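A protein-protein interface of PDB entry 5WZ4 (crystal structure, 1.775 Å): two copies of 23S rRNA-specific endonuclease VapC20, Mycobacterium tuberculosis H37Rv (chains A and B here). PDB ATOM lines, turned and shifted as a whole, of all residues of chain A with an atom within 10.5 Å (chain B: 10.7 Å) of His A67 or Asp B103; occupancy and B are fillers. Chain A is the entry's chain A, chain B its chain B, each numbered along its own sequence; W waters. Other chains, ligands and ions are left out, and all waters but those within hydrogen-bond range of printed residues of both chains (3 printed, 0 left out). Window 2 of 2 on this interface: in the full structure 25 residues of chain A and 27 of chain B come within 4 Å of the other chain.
Water W3 bridges OG1 of Thr A59 and N of Phe B109. Water W1 lies within hydrogen-bond range of the backbone carbonyl oxygen of Arg B105, the backbone NH of Tyr B107 and the side-chain amide nitrogen of Asn A62. Water W2 bridges NE of Arg A63 and OE2 of Glu B106.
Among the printed residues, merely in contact across the chains: Ala A74 with Trp B96 (3.5 Å), His A67 with Asp B103 (3.5 Å), Trp A58 with Leu B99 (3.6 Å), Thr A59 with Ser B108 (3.6 Å), Trp A58 with Phe B109 (3.7 Å), Asn A62 with Glu B106 (3.7 Å), Trp A58 with Trp B96 (3.8 Å) and His A67 with His B102 (3.8 Å).
No position is printed for both chains. Of the 14 pairs that touch across the chains among the printed residues, none has its exchanged pair printed and touching as well.
A ring nitrogen (NE2) of His A67 sits close to the backbone carbonyl oxygen (O) of Val B100 (3.3 Å). A ring nitrogen (NE2) of His A67 lies within hydrogen-bond range of the backbone carbonyl oxygen of Leu B99 (2.7 Å). The side-chain carboxylate of Glu B106 is in salt-bridge range of the guanidinium group of Arg A63 (3.7 Å). The indole nitrogen (NE1) of Trp A58 lies within hydrogen-bond range of the backbone carbonyl oxygen (O) of Tyr B107. The backbone NH of Phe B109 sits at hydrogen-bond distance from the side-chain hydroxyl of Thr A59, at 3.0 Å. ND2 of Asn A62 is in hydrogen-bond range of O of Tyr B107 (3.1 Å).
The side-chain amide oxygen (OD1) of Asn A62 is in hydrogen-bond range of the backbone NH (N) of His A67 (3.3 Å). The backbone carbonyl oxygen of Trp B98 is in hydrogen-bond range of a ring nitrogen (ND1) of His B102 (3.1 Å).
Of the printed residues of chain B, Arg A63 touches Glu B106 (3.2 Å). No residue of chain B comes within 4 Å of Gly A66. No residue of chain B comes within 4 Å of Ala A69. No residue of chain B comes within 4 Å of Ala A70. No residue of chain B comes within 4 Å of Val A71. Ala A75 touches none of the printed residues of chain B. Of the printed residues of chain A, Leu B99 touches Trp A58 and His A67. Val B100 touches just one residue of chain A: His A67 (3.0 Å). Asp B103 touches one residue of chain A. No residue of chain A comes within 4 Å of Glu B104. Of the printed residues of chain A, Ser B108 touches Thr A59. The nearest residue of chain B that does not touch His A67 is Arg B101 (4.7 Å). The nearest residue of chain A that does not touch Asp B103 is Arg A68 (6.5 Å). The nearest printed residue of chain A that does not touch Ser B108 is Trp A58 (4.1 Å).
Printed residues of chain A that touch a printed residue of chain B: Trp A58, Thr A59, Asn A62, Arg A63, His A67 and Ala A74. Hydrophobic or aromatic side chains of chain A within 4 Å of the printed part of chain B: Trp A58, His A67 and Ala A74. Of the 16 printed residues of chain B, 9 touch a printed residue of chain A. Among the printed residues, 14 pairs touch across the chains.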
ATOM      1  N   GLY A  26     -19.127  -7.214  10.593  1.00  0.00           N
ATOM      2  CA  GLY A  26     -19.691  -7.401  11.919  1.00  0.00           C
ATOM      3  C   GLY A  26     -19.977  -6.119  12.680  1.00  0.00           C
ATOM      4  O   GLY A  26     -20.417  -6.157  13.829  1.00  0.00           O
ATOM      5  N   THR A  57     -10.137 -10.294  15.050  1.00  0.00           N
ATOM      6  CA  THR A  57     -11.464  -9.740  14.809  1.00  0.00           C
ATOM      7  C   THR A  57     -12.228  -9.554  16.114  1.00  0.00           C
ATOM      8  O   THR A  57     -12.855  -8.516  16.323  1.00  0.00           O
ATOM      9  CB  THR A  57     -12.275 -10.636  13.859  1.00  0.00           C
ATOM     10  OG1 THR A  57     -11.654 -10.637  12.569  1.00  0.00           O
ATOM     11  CG2 THR A  57     -13.698 -10.124  13.723  1.00  0.00           C
ATOM     12  N   TRP A  58     -12.174 -10.563  16.984  1.00  0.00           N
ATOM     13  CA  TRP A  58     -12.754 -10.453  18.320  1.00  0.00           C
ATOM     14  C   TRP A  58     -12.268  -9.191  19.006  1.00  0.00           C
ATOM     15  O   TRP A  58     -13.065  -8.378  19.475  1.00  0.00           O
ATOM     16  CB  TRP A  58     -12.398 -11.661  19.201  1.00  0.00           C
ATOM     17  CG  TRP A  58     -12.624 -11.370  20.670  1.00  0.00           C
ATOM     18  CD1 TRP A  58     -11.745 -10.779  21.538  1.00  0.00           C
ATOM     19  CD2 TRP A  58     -13.816 -11.629  21.425  1.00  0.00           C
ATOM     20  NE1 TRP A  58     -12.317 -10.656  22.782  1.00  0.00           N
ATOM     21  CE2 TRP A  58     -13.585 -11.175  22.741  1.00  0.00           C
ATOM     22  CE3 TRP A  58     -15.051 -12.210  21.120  1.00  0.00           C
ATOM     23  CZ2 TRP A  58     -14.542 -11.280  23.746  1.00  0.00           C
ATOM     24  CZ3 TRP A  58     -16.002 -12.313  22.122  1.00  0.00           C
ATOM     25  CH2 TRP A  58     -15.739 -11.852  23.419  1.00  0.00           C
ATOM     26  N   THR A  59     -10.948  -9.051  19.075  1.00  0.00           N
ATOM     27  CA  THR A  59     -10.320  -7.964  19.811  1.00  0.00           C
ATOM     28  C   THR A  59     -10.741  -6.612  19.259  1.00  0.00           C
ATOM     29  O   THR A  59     -11.078  -5.702  20.014  1.00  0.00           O
ATOM     30  CB  THR A  59      -8.789  -8.084  19.773  1.00  0.00           C
ATOM     31  OG1 THR A  59      -8.398  -9.314  20.395  1.00  0.00           O
ATOM     32  CG2 THR A  59      -8.135  -6.916  20.503  1.00  0.00           C
ATOM     33  N   LEU A  60     -10.739  -6.501  17.936  1.00  0.00           N
ATOM     34  CA  LEU A  60     -11.105  -5.262  17.268  1.00  0.00           C
ATOM     35  C   LEU A  60     -12.569  -4.900  17.518  1.00  0.00           C
ATOM     36  O   LEU A  60     -12.878  -3.766  17.880  1.00  0.00           O
ATOM     37  CB  LEU A  60     -10.838  -5.375  15.766  1.00  0.00           C
ATOM     38  CG  LEU A  60     -10.661  -4.055  15.015  1.00  0.00           C
ATOM     39  CD1 LEU A  60      -9.590  -3.207  15.682  1.00  0.00           C
ATOM     40  CD2 LEU A  60     -10.323  -4.312  13.555  1.00  0.00           C
ATOM     41  N   LEU A  61     -13.464  -5.866  17.332  1.00  0.00           N
ATOM     42  CA  LEU A  61     -14.892  -5.627  17.524  1.00  0.00           C
ATOM     43  C   LEU A  61     -15.230  -5.394  18.992  1.00  0.00           C
ATOM     44  O   LEU A  61     -16.148  -4.642  19.311  1.00  0.00           O
ATOM     45  CB  LEU A  61     -15.715  -6.795  16.980  1.00  0.00           C
ATOM     46  CG  LEU A  61     -15.778  -6.932  15.459  1.00  0.00           C
ATOM     47  CD1 LEU A  61     -16.621  -8.135  15.064  1.00  0.00           C
ATOM     48  CD2 LEU A  61     -16.324  -5.663  14.829  1.00  0.00           C
ATOM     49  N   ASN A  62     -14.486  -6.044  19.884  1.00  0.00           N
ATOM     50  CA  ASN A  62     -14.680  -5.840  21.314  1.00  0.00           C
ATOM     51  C   ASN A  62     -14.297  -4.418  21.714  1.00  0.00           C
ATOM     52  O   ASN A  62     -15.018  -3.763  22.468  1.00  0.00           O
ATOM     53  CB  ASN A  62     -13.866  -6.853  22.124  1.00  0.00           C
ATOM     54  CG  ASN A  62     -14.390  -7.025  23.541  1.00  0.00           C
ATOM     55  OD1 ASN A  62     -15.558  -6.759  23.821  1.00  0.00           O
ATOM     56  ND2 ASN A  62     -13.525  -7.481  24.438  1.00  0.00           N
ATOM     57  N   ARG A  63     -13.166  -3.941  21.198  1.00  0.00           N
ATOM     58  CA  ARG A  63     -12.700  -2.585  21.491  1.00  0.00           C
ATOM     59  C   ARG A  63     -13.609  -1.525  20.881  1.00  0.00           C
ATOM     60  O   ARG A  63     -13.757  -0.433  21.432  1.00  0.00           O
ATOM     61  CB  ARG A  63     -11.270  -2.368  20.981  1.00  0.00           C
ATOM     62  CG  ARG A  63     -10.208  -3.230  21.645  1.00  0.00           C
ATOM     63  CD  ARG A  63      -8.843  -2.563  21.599  1.00  0.00           C
ATOM     64  NE  ARG A  63      -7.837  -3.329  22.334  1.00  0.00           N
ATOM     65  CZ  ARG A  63      -6.787  -3.916  21.769  1.00  0.00           C
ATOM     66  NH1 ARG A  63      -6.595  -3.821  20.461  1.00  0.00           N
ATOM     67  NH2 ARG A  63      -5.924  -4.594  22.515  1.00  0.00           N
ATOM     68  N   ARG A  64     -14.220  -1.853  19.746  1.00  0.00           N
ATOM     69  CA  ARG A  64     -15.001  -0.884  18.987  1.00  0.00           C
ATOM     70  C   ARG A  64     -16.495  -0.933  19.306  1.00  0.00           C
ATOM     71  O   ARG A  64     -17.122   0.102  19.522  1.00  0.00           O
ATOM     72  CB  ARG A  64     -14.782  -1.100  17.490  1.00  0.00           C
ATOM     73  CG  ARG A  64     -15.517  -0.115  16.605  1.00  0.00           C
ATOM     74  CD  ARG A  64     -14.725   0.171  15.343  1.00  0.00           C
ATOM     75  NE  ARG A  64     -15.321   1.243  14.555  1.00  0.00           N
ATOM     76  CZ  ARG A  64     -14.862   1.643  13.374  1.00  0.00           C
ATOM     77  NH1 ARG A  64     -13.795   1.062  12.844  1.00  0.00           N
ATOM     78  NH2 ARG A  64     -15.468   2.627  12.725  1.00  0.00           N
ATOM     79  N   CSO A  65     -17.069  -2.133  19.332  1.00  0.00           N
ATOM     80  CA  CSO A  65     -18.509  -2.259  19.572  1.00  0.00           C
ATOM     81  CB  CSO A  65     -19.227  -2.864  18.363  1.00  0.00           C
ATOM     82  SG  CSO A  65     -18.936  -1.841  16.911  1.00  0.00           S
ATOM     83  C   CSO A  65     -18.930  -2.985  20.845  1.00  0.00           C
ATOM     84  O   CSO A  65     -20.123  -3.133  21.109  1.00  0.00           O
ATOM     85  OD  CSO A  65     -20.390  -0.861  16.588  1.00  0.00           O
ATOM     86  N   GLY A  66     -17.963  -3.431  21.634  1.00  0.00           N
ATOM     87  CA  GLY A  66     -18.282  -4.074  22.891  1.00  0.00           C
ATOM     88  C   GLY A  66     -18.470  -5.571  22.767  1.00  0.00           C
ATOM     89  O   GLY A  66     -18.336  -6.139  21.684  1.00  0.00           O
ATOM     90  N   HIS A  67     -18.812  -6.198  23.888  1.00  0.00           N
ATOM     91  CA  HIS A  67     -18.782  -7.652  24.027  1.00  0.00           C
ATOM     92  C   HIS A  67     -19.763  -8.394  23.116  1.00  0.00           C
ATOM     93  O   HIS A  67     -19.402  -9.403  22.507  1.00  0.00           O
ATOM     94  CB  HIS A  67     -19.054  -8.027  25.489  1.00  0.00           C
ATOM     95  CG  HIS A  67     -18.824  -9.472  25.796  1.00  0.00           C
ATOM     96  ND1 HIS A  67     -19.824 -10.415  25.720  1.00  0.00           N
ATOM     97  CD2 HIS A  67     -17.709 -10.134  26.184  1.00  0.00           C
ATOM     98  CE1 HIS A  67     -19.334 -11.599  26.043  1.00  0.00           C
ATOM     99  NE2 HIS A  67     -18.053 -11.457  26.328  1.00  0.00           N
ATOM    100  N   ARG A  68     -20.996  -7.903  23.026  1.00  0.00           N
ATOM    101  CA  ARG A  68     -22.038  -8.597  22.272  1.00  0.00           C
ATOM    102  C   ARG A  68     -21.673  -8.738  20.798  1.00  0.00           C
ATOM    103  O   ARG A  68     -21.817  -9.813  20.215  1.00  0.00           O
ATOM    104  CB  ARG A  68     -23.377  -7.871  22.413  1.00  0.00           C
ATOM    105  CG  ARG A  68     -24.560  -8.633  21.830  1.00  0.00           C
ATOM    106  CD  ARG A  68     -25.874  -7.936  22.154  1.00  0.00           C
ATOM    107  NE  ARG A  68     -27.035  -8.715  21.730  1.00  0.00           N
ATOM    108  CZ  ARG A  68     -27.645  -8.574  20.559  1.00  0.00           C
ATOM    109  NH1 ARG A  68     -27.204  -7.685  19.678  1.00  0.00           N
ATOM    110  NH2 ARG A  68     -28.695  -9.328  20.262  1.00  0.00           N
ATOM    111  N   ALA A  69     -21.192  -7.651  20.205  1.00  0.00           N
ATOM    112  CA  ALA A  69     -20.788  -7.655  18.803  1.00  0.00           C
ATOM    113  C   ALA A  69     -19.596  -8.579  18.577  1.00  0.00           C
ATOM    114  O   ALA A  69     -19.465  -9.204  17.523  1.00  0.00           O
ATOM    115  CB  ALA A  69     -20.456  -6.246  18.349  1.00  0.00           C
ATOM    116  N   ALA A  70     -18.730  -8.661  19.580  1.00  0.00           N
ATOM    117  CA  ALA A  70     -17.545  -9.504  19.508  1.00  0.00           C
ATOM    118  C   ALA A  70     -17.914 -10.989  19.552  1.00  0.00           C
ATOM    119  O   ALA A  70     -17.292 -11.807  18.878  1.00  0.00           O
ATOM    120  CB  ALA A  70     -16.588  -9.157  20.633  1.00  0.00           C
ATOM    121  N   VAL A  71     -18.937 -11.324  20.332  1.00  0.00           N
ATOM    122  CA  VAL A  71     -19.406 -12.706  20.449  1.00  0.00           C
ATOM    123  C   VAL A  71     -19.758 -13.296  19.076  1.00  0.00           C
ATOM    124  O   VAL A  71     -19.553 -14.488  18.827  1.00  0.00           O
ATOM    125  CB  VAL A  71     -20.622 -12.797  21.403  1.00  0.00           C
ATOM    126  CG1 VAL A  71     -21.320 -14.147  21.291  1.00  0.00           C
ATOM    127  CG2 VAL A  71     -20.184 -12.547  22.835  1.00  0.00           C
ATOM    128  N   ALA A  72     -20.257 -12.450  18.179  1.00  0.00           N
ATOM    129  CA  ALA A  72     -20.558 -12.868  16.812  1.00  0.00           C
ATOM    130  C   ALA A  72     -19.321 -13.422  16.106  1.00  0.00           C
ATOM    131  O   ALA A  72     -19.399 -14.420  15.387  1.00  0.00           O
ATOM    132  CB  ALA A  72     -21.137 -11.707  16.021  1.00  0.00           C
ATOM    133  N   ALA A  73     -18.181 -12.772  16.319  1.00  0.00           N
ATOM    134  CA  ALA A  73     -16.922 -13.224  15.738  1.00  0.00           C
ATOM    135  C   ALA A  73     -16.502 -14.568  16.322  1.00  0.00           C
ATOM    136  O   ALA A  73     -16.012 -15.444  15.607  1.00  0.00           O
ATOM    137  CB  ALA A  73     -15.833 -12.187  15.959  1.00  0.00           C
ATOM    138  N   ALA A  74     -16.699 -14.725  17.627  1.00  0.00           N
ATOM    139  CA  ALA A  74     -16.390 -15.975  18.304  1.00  0.00           C
ATOM    140  C   ALA A  74     -17.173 -17.132  17.692  1.00  0.00           C
ATOM    141  O   ALA A  74     -16.685 -18.258  17.616  1.00  0.00           O
ATOM    142  CB  ALA A  74     -16.690 -15.862  19.791  1.00  0.00           C
ATOM    143  N   ALA A  75     -18.390 -16.840  17.252  1.00  0.00           N
ATOM    144  CA  ALA A  75     -19.293 -17.869  16.753  1.00  0.00           C
ATOM    145  C   ALA A  75     -18.930 -18.353  15.354  1.00  0.00           C
ATOM    146  O   ALA A  75     -19.400 -19.404  14.920  1.00  0.00           O
ATOM    147  CB  ALA A  75     -20.702 -17.356  16.766  1.00  0.00           C
ATOM    148  N   ALA B  95     -10.211 -20.543  25.558  1.00  0.00           N
ATOM    149  CA  ALA B  95     -10.135 -19.088  25.579  1.00  0.00           C
ATOM    150  C   ALA B  95     -11.410 -18.467  25.012  1.00  0.00           C
ATOM    151  O   ALA B  95     -11.915 -17.477  25.540  1.00  0.00           O
ATOM    152  CB  ALA B  95      -8.917 -18.607  24.801  1.00  0.00           C
ATOM    153  N   TRP B  96     -11.925 -19.050  23.935  1.00  0.00           N
ATOM    154  CA  TRP B  96     -13.153 -18.552  23.323  1.00  0.00           C
ATOM    155  C   TRP B  96     -14.329 -18.630  24.289  1.00  0.00           C
ATOM    156  O   TRP B  96     -15.068 -17.662  24.458  1.00  0.00           O
ATOM    157  CB  TRP B  96     -13.481 -19.331  22.050  1.00  0.00           C
ATOM    158  CG  TRP B  96     -12.686 -18.907  20.843  1.00  0.00           C
ATOM    159  CD1 TRP B  96     -11.828 -19.681  20.114  1.00  0.00           C
ATOM    160  CD2 TRP B  96     -12.685 -17.614  20.220  1.00  0.00           C
ATOM    161  NE1 TRP B  96     -11.296 -18.950  19.076  1.00  0.00           N
ATOM    162  CE2 TRP B  96     -11.806 -17.680  19.121  1.00  0.00           C
ATOM    163  CE3 TRP B  96     -13.342 -16.409  20.487  1.00  0.00           C
ATOM    164  CZ2 TRP B  96     -11.568 -16.589  18.289  1.00  0.00           C
ATOM    165  CZ3 TRP B  96     -13.103 -15.326  19.661  1.00  0.00           C
ATOM    166  CH2 TRP B  96     -12.221 -15.424  18.574  1.00  0.00           C
ATOM    167  N   GLU B  97     -14.501 -19.786  24.920  1.00  0.00           N
ATOM    168  CA  GLU B  97     -15.599 -19.973  25.860  1.00  0.00           C
ATOM    169  C   GLU B  97     -15.456 -19.016  27.038  1.00  0.00           C
ATOM    170  O   GLU B  97     -16.442 -18.491  27.549  1.00  0.00           O
ATOM    171  CB  GLU B  97     -15.650 -21.422  26.344  1.00  0.00           C
ATOM    172  CG  GLU B  97     -16.007 -22.417  25.249  1.00  0.00           C
ATOM    173  CD  GLU B  97     -15.932 -23.856  25.715  1.00  0.00           C
ATOM    174  OE1 GLU B  97     -15.366 -24.102  26.801  1.00  0.00           O
ATOM    175  OE2 GLU B  97     -16.438 -24.742  24.992  1.00  0.00           O
ATOM    176  N   TRP B  98     -14.214 -18.782  27.446  1.00  0.00           N
ATOM    177  CA  TRP B  98     -13.915 -17.847  28.522  1.00  0.00           C
ATOM    178  C   TRP B  98     -14.276 -16.419  28.121  1.00  0.00           C
ATOM    179  O   TRP B  98     -14.893 -15.688  28.896  1.00  0.00           O
ATOM    180  CB  TRP B  98     -12.435 -17.940  28.903  1.00  0.00           C
ATOM    181  CG  TRP B  98     -12.074 -17.166  30.131  1.00  0.00           C
ATOM    182  CD1 TRP B  98     -12.052 -17.630  31.415  1.00  0.00           C
ATOM    183  CD2 TRP B  98     -11.679 -15.793  30.193  1.00  0.00           C
ATOM    184  NE1 TRP B  98     -11.667 -16.628  32.273  1.00  0.00           N
ATOM    185  CE2 TRP B  98     -11.434 -15.489  31.546  1.00  0.00           C
ATOM    186  CE3 TRP B  98     -11.511 -14.788  29.234  1.00  0.00           C
ATOM    187  CZ2 TRP B  98     -11.029 -14.225  31.965  1.00  0.00           C
ATOM    188  CZ3 TRP B  98     -11.110 -13.534  29.653  1.00  0.00           C
ATOM    189  CH2 TRP B  98     -10.873 -13.264  31.007  1.00  0.00           C
ATOM    190  N   LEU B  99     -13.891 -16.031  26.907  1.00  0.00           N
ATOM    191  CA  LEU B  99     -14.192 -14.697  26.385  1.00  0.00           C
ATOM    192  C   LEU B  99     -15.688 -14.421  26.307  1.00  0.00           C
ATOM    193  O   LEU B  99     -16.148 -13.329  26.646  1.00  0.00           O
ATOM    194  CB  LEU B  99     -13.579 -14.517  24.998  1.00  0.00           C
ATOM    195  CG  LEU B  99     -12.084 -14.205  24.950  1.00  0.00           C
ATOM    196  CD1 LEU B  99     -11.578 -14.288  23.522  1.00  0.00           C
ATOM    197  CD2 LEU B  99     -11.806 -12.832  25.548  1.00  0.00           C
ATOM    198  N   VAL B 100     -16.442 -15.412  25.845  1.00  0.00           N
ATOM    199  CA  VAL B 100     -17.887 -15.272  25.725  1.00  0.00           C
ATOM    200  C   VAL B 100     -18.509 -15.092  27.107  1.00  0.00           C
ATOM    201  O   VAL B 100     -19.448 -14.315  27.280  1.00  0.00           O
ATOM    202  CB  VAL B 100     -18.510 -16.493  25.013  1.00  0.00           C
ATOM    203  CG1 VAL B 100     -20.031 -16.417  25.031  1.00  0.00           C
ATOM    204  CG2 VAL B 100     -18.002 -16.586  23.586  1.00  0.00           C
ATOM    205  N   ARG B 101     -17.958 -15.793  28.094  1.00  0.00           N
ATOM    206  CA  ARG B 101     -18.468 -15.744  29.463  1.00  0.00           C
ATOM    207  C   ARG B 101     -18.202 -14.417  30.165  1.00  0.00           C
ATOM    208  O   ARG B 101     -19.049 -13.921  30.907  1.00  0.00           O
ATOM    209  CB  ARG B 101     -17.857 -16.874  30.297  1.00  0.00           C
ATOM    210  CG  ARG B 101     -18.810 -18.013  30.604  1.00  0.00           C
ATOM    211  CD  ARG B 101     -18.193 -19.007  31.582  1.00  0.00           C
ATOM    212  NE  ARG B 101     -17.191 -19.857  30.945  1.00  0.00           N
ATOM    213  CZ  ARG B 101     -15.907 -19.892  31.291  1.00  0.00           C
ATOM    214  NH1 ARG B 101     -15.458 -19.122  32.274  1.00  0.00           N
ATOM    215  NH2 ARG B 101     -15.072 -20.701  30.653  1.00  0.00           N
ATOM    216  N   HIS B 102     -17.024 -13.846  29.940  1.00  0.00           N
ATOM    217  CA  HIS B 102     -16.577 -12.711  30.740  1.00  0.00           C
ATOM    218  C   HIS B 102     -16.836 -11.363  30.081  1.00  0.00           C
ATOM    219  O   HIS B 102     -15.929 -10.739  29.529  1.00  0.00           O
ATOM    220  CB  HIS B 102     -15.092 -12.861  31.067  1.00  0.00           C
ATOM    221  CG  HIS B 102     -14.821 -13.856  32.150  1.00  0.00           C
ATOM    222  ND1 HIS B 102     -14.767 -15.214  31.919  1.00  0.00           N
ATOM    223  CD2 HIS B 102     -14.621 -13.693  33.481  1.00  0.00           C
ATOM    224  CE1 HIS B 102     -14.529 -15.843  33.056  1.00  0.00           C
ATOM    225  NE2 HIS B 102     -14.435 -14.943  34.019  1.00  0.00           N
ATOM    226  N   ASP B 103     -18.083 -10.911  30.169  1.00  0.00           N
ATOM    227  CA  ASP B 103     -18.488  -9.644  29.573  1.00  0.00           C
ATOM    228  C   ASP B 103     -18.262  -8.472  30.523  1.00  0.00           C
ATOM    229  O   ASP B 103     -18.442  -7.317  30.146  1.00  0.00           O
ATOM    230  CB  ASP B 103     -19.962  -9.704  29.155  1.00  0.00           C
ATOM    231  CG  ASP B 103     -20.894  -9.921  30.335  1.00  0.00           C
ATOM    232  OD1 ASP B 103     -20.526 -10.673  31.260  1.00  0.00           O
ATOM    233  OD2 ASP B 103     -21.999  -9.341  30.336  1.00  0.00           O
ATOM    234  N   GLU B 104     -17.852  -8.773  31.753  1.00  0.00           N
ATOM    235  CA  GLU B 104     -17.733  -7.746  32.786  1.00  0.00           C
ATOM    236  C   GLU B 104     -16.537  -6.823  32.569  1.00  0.00           C
ATOM    237  O   GLU B 104     -16.407  -5.799  33.238  1.00  0.00           O
ATOM    238  CB  GLU B 104     -17.641  -8.394  34.172  1.00  0.00           C
ATOM    239  CG  GLU B 104     -16.263  -8.937  34.528  1.00  0.00           C
ATOM    240  CD  GLU B 104     -15.986 -10.295  33.912  1.00  0.00           C
ATOM    241  OE1 GLU B 104     -16.935 -10.930  33.409  1.00  0.00           O
ATOM    242  OE2 GLU B 104     -14.816 -10.728  33.937  1.00  0.00           O
ATOM    243  N   ARG B 105     -15.666  -7.186  31.636  1.00  0.00           N
ATOM    244  CA  ARG B 105     -14.470  -6.398  31.363  1.00  0.00           C
ATOM    245  C   ARG B 105     -13.989  -6.653  29.937  1.00  0.00           C
ATOM    246  O   ARG B 105     -14.220  -7.728  29.383  1.00  0.00           O
ATOM    247  CB  ARG B 105     -13.368  -6.729  32.378  1.00  0.00           C
ATOM    248  CG  ARG B 105     -12.132  -5.846  32.288  1.00  0.00           C
ATOM    249  CD  ARG B 105     -11.115  -6.191  33.364  1.00  0.00           C
ATOM    250  NE  ARG B 105      -9.818  -5.577  33.098  1.00  0.00           N
ATOM    251  CZ  ARG B 105      -9.260  -4.648  33.866  1.00  0.00           C
ATOM    252  NH1 ARG B 105      -9.883  -4.227  34.958  1.00  0.00           N
ATOM    253  NH2 ARG B 105      -8.077  -4.143  33.545  1.00  0.00           N
ATOM    254  N   GLU B 106     -13.336  -5.660  29.339  1.00  0.00           N
ATOM    255  CA  GLU B 106     -12.816  -5.796  27.983  1.00  0.00           C
ATOM    256  C   GLU B 106     -11.523  -6.605  27.957  1.00  0.00           C
ATOM    257  O   GLU B 106     -10.487  -6.150  28.441  1.00  0.00           O
ATOM    258  CB  GLU B 106     -12.578  -4.424  27.356  1.00  0.00           C
ATOM    259  CG  GLU B 106     -11.948  -4.488  25.974  1.00  0.00           C
ATOM    260  CD  GLU B 106     -11.715  -3.118  25.374  1.00  0.00           C
ATOM    261  OE1 GLU B 106     -12.589  -2.240  25.530  1.00  0.00           O
ATOM    262  OE2 GLU B 106     -10.652  -2.916  24.752  1.00  0.00           O
ATOM    263  N   TYR B 107     -11.597  -7.802  27.384  1.00  0.00           N
ATOM    264  CA  TYR B 107     -10.439  -8.683  27.256  1.00  0.00           C
ATOM    265  C   TYR B 107     -10.131  -8.964  25.789  1.00  0.00           C
ATOM    266  O   TYR B 107     -11.038  -9.213  24.996  1.00  0.00           O
ATOM    267  CB  TYR B 107     -10.677 -10.005  27.987  1.00  0.00           C
ATOM    268  CG  TYR B 107     -10.670  -9.928  29.499  1.00  0.00           C
ATOM    269  CD1 TYR B 107      -9.484  -9.760  30.202  1.00  0.00           C
ATOM    270  CD2 TYR B 107     -11.848 -10.057  30.225  1.00  0.00           C
ATOM    271  CE1 TYR B 107      -9.472  -9.704  31.585  1.00  0.00           C
ATOM    272  CE2 TYR B 107     -11.845 -10.003  31.610  1.00  0.00           C
ATOM    273  CZ  TYR B 107     -10.654  -9.826  32.283  1.00  0.00           C
ATOM    274  OH  TYR B 107     -10.642  -9.772  33.657  1.00  0.00           O
ATOM    275  N   SER B 108      -8.853  -8.935  25.431  1.00  0.00           N
ATOM    276  CA  SER B 108      -8.446  -9.281  24.075  1.00  0.00           C
ATOM    277  C   SER B 108      -8.373 -10.795  23.924  1.00  0.00           C
ATOM    278  O   SER B 108      -8.380 -11.528  24.913  1.00  0.00           O
ATOM    279  CB  SER B 108      -7.094  -8.657  23.734  1.00  0.00           C
ATOM    280  OG  SER B 108      -6.059  -9.285  24.466  1.00  0.00           O
ATOM    281  N   PHE B 109      -8.298 -11.257  22.681  1.00  0.00           N
ATOM    282  CA  PHE B 109      -8.159 -12.679  22.409  1.00  0.00           C
ATOM    283  C   PHE B 109      -6.796 -13.205  22.856  1.00  0.00           C
ATOM    284  O   PHE B 109      -6.708 -14.270  23.466  1.00  0.00           O
ATOM    285  CB  PHE B 109      -8.368 -12.959  20.922  1.00  0.00           C
ATOM    286  CG  PHE B 109      -8.092 -14.382  20.529  1.00  0.00           C
ATOM    287  CD1 PHE B 109      -9.032 -15.372  20.752  1.00  0.00           C
ATOM    288  CD2 PHE B 109      -6.889 -14.727  19.932  1.00  0.00           C
ATOM    289  CE1 PHE B 109      -8.777 -16.682  20.390  1.00  0.00           C
ATOM    290  CE2 PHE B 109      -6.630 -16.028  19.564  1.00  0.00           C
ATOM    291  CZ  PHE B 109      -7.576 -17.008  19.793  1.00  0.00           C
ATOM    292  N   ALA B 112      -6.694 -13.672  26.438  1.00  0.00           N
ATOM    293  CA  ALA B 112      -7.528 -14.808  26.805  1.00  0.00           C
ATOM    294  C   ALA B 112      -6.776 -16.122  26.627  1.00  0.00           C
ATOM    295  O   ALA B 112      -6.844 -17.002  27.483  1.00  0.00           O
ATOM    296  CB  ALA B 112      -8.797 -14.818  25.988  1.00  0.00           C
HETATM  297  O   HOH W   1     -14.265  -8.816  26.944  1.00  0.00           O
HETATM  298  O   HOH W   2      -8.765  -5.110  24.367  1.00  0.00           O
HETATM  299  O   HOH W   3      -5.983 -10.056  20.589  1.00  0.00           O
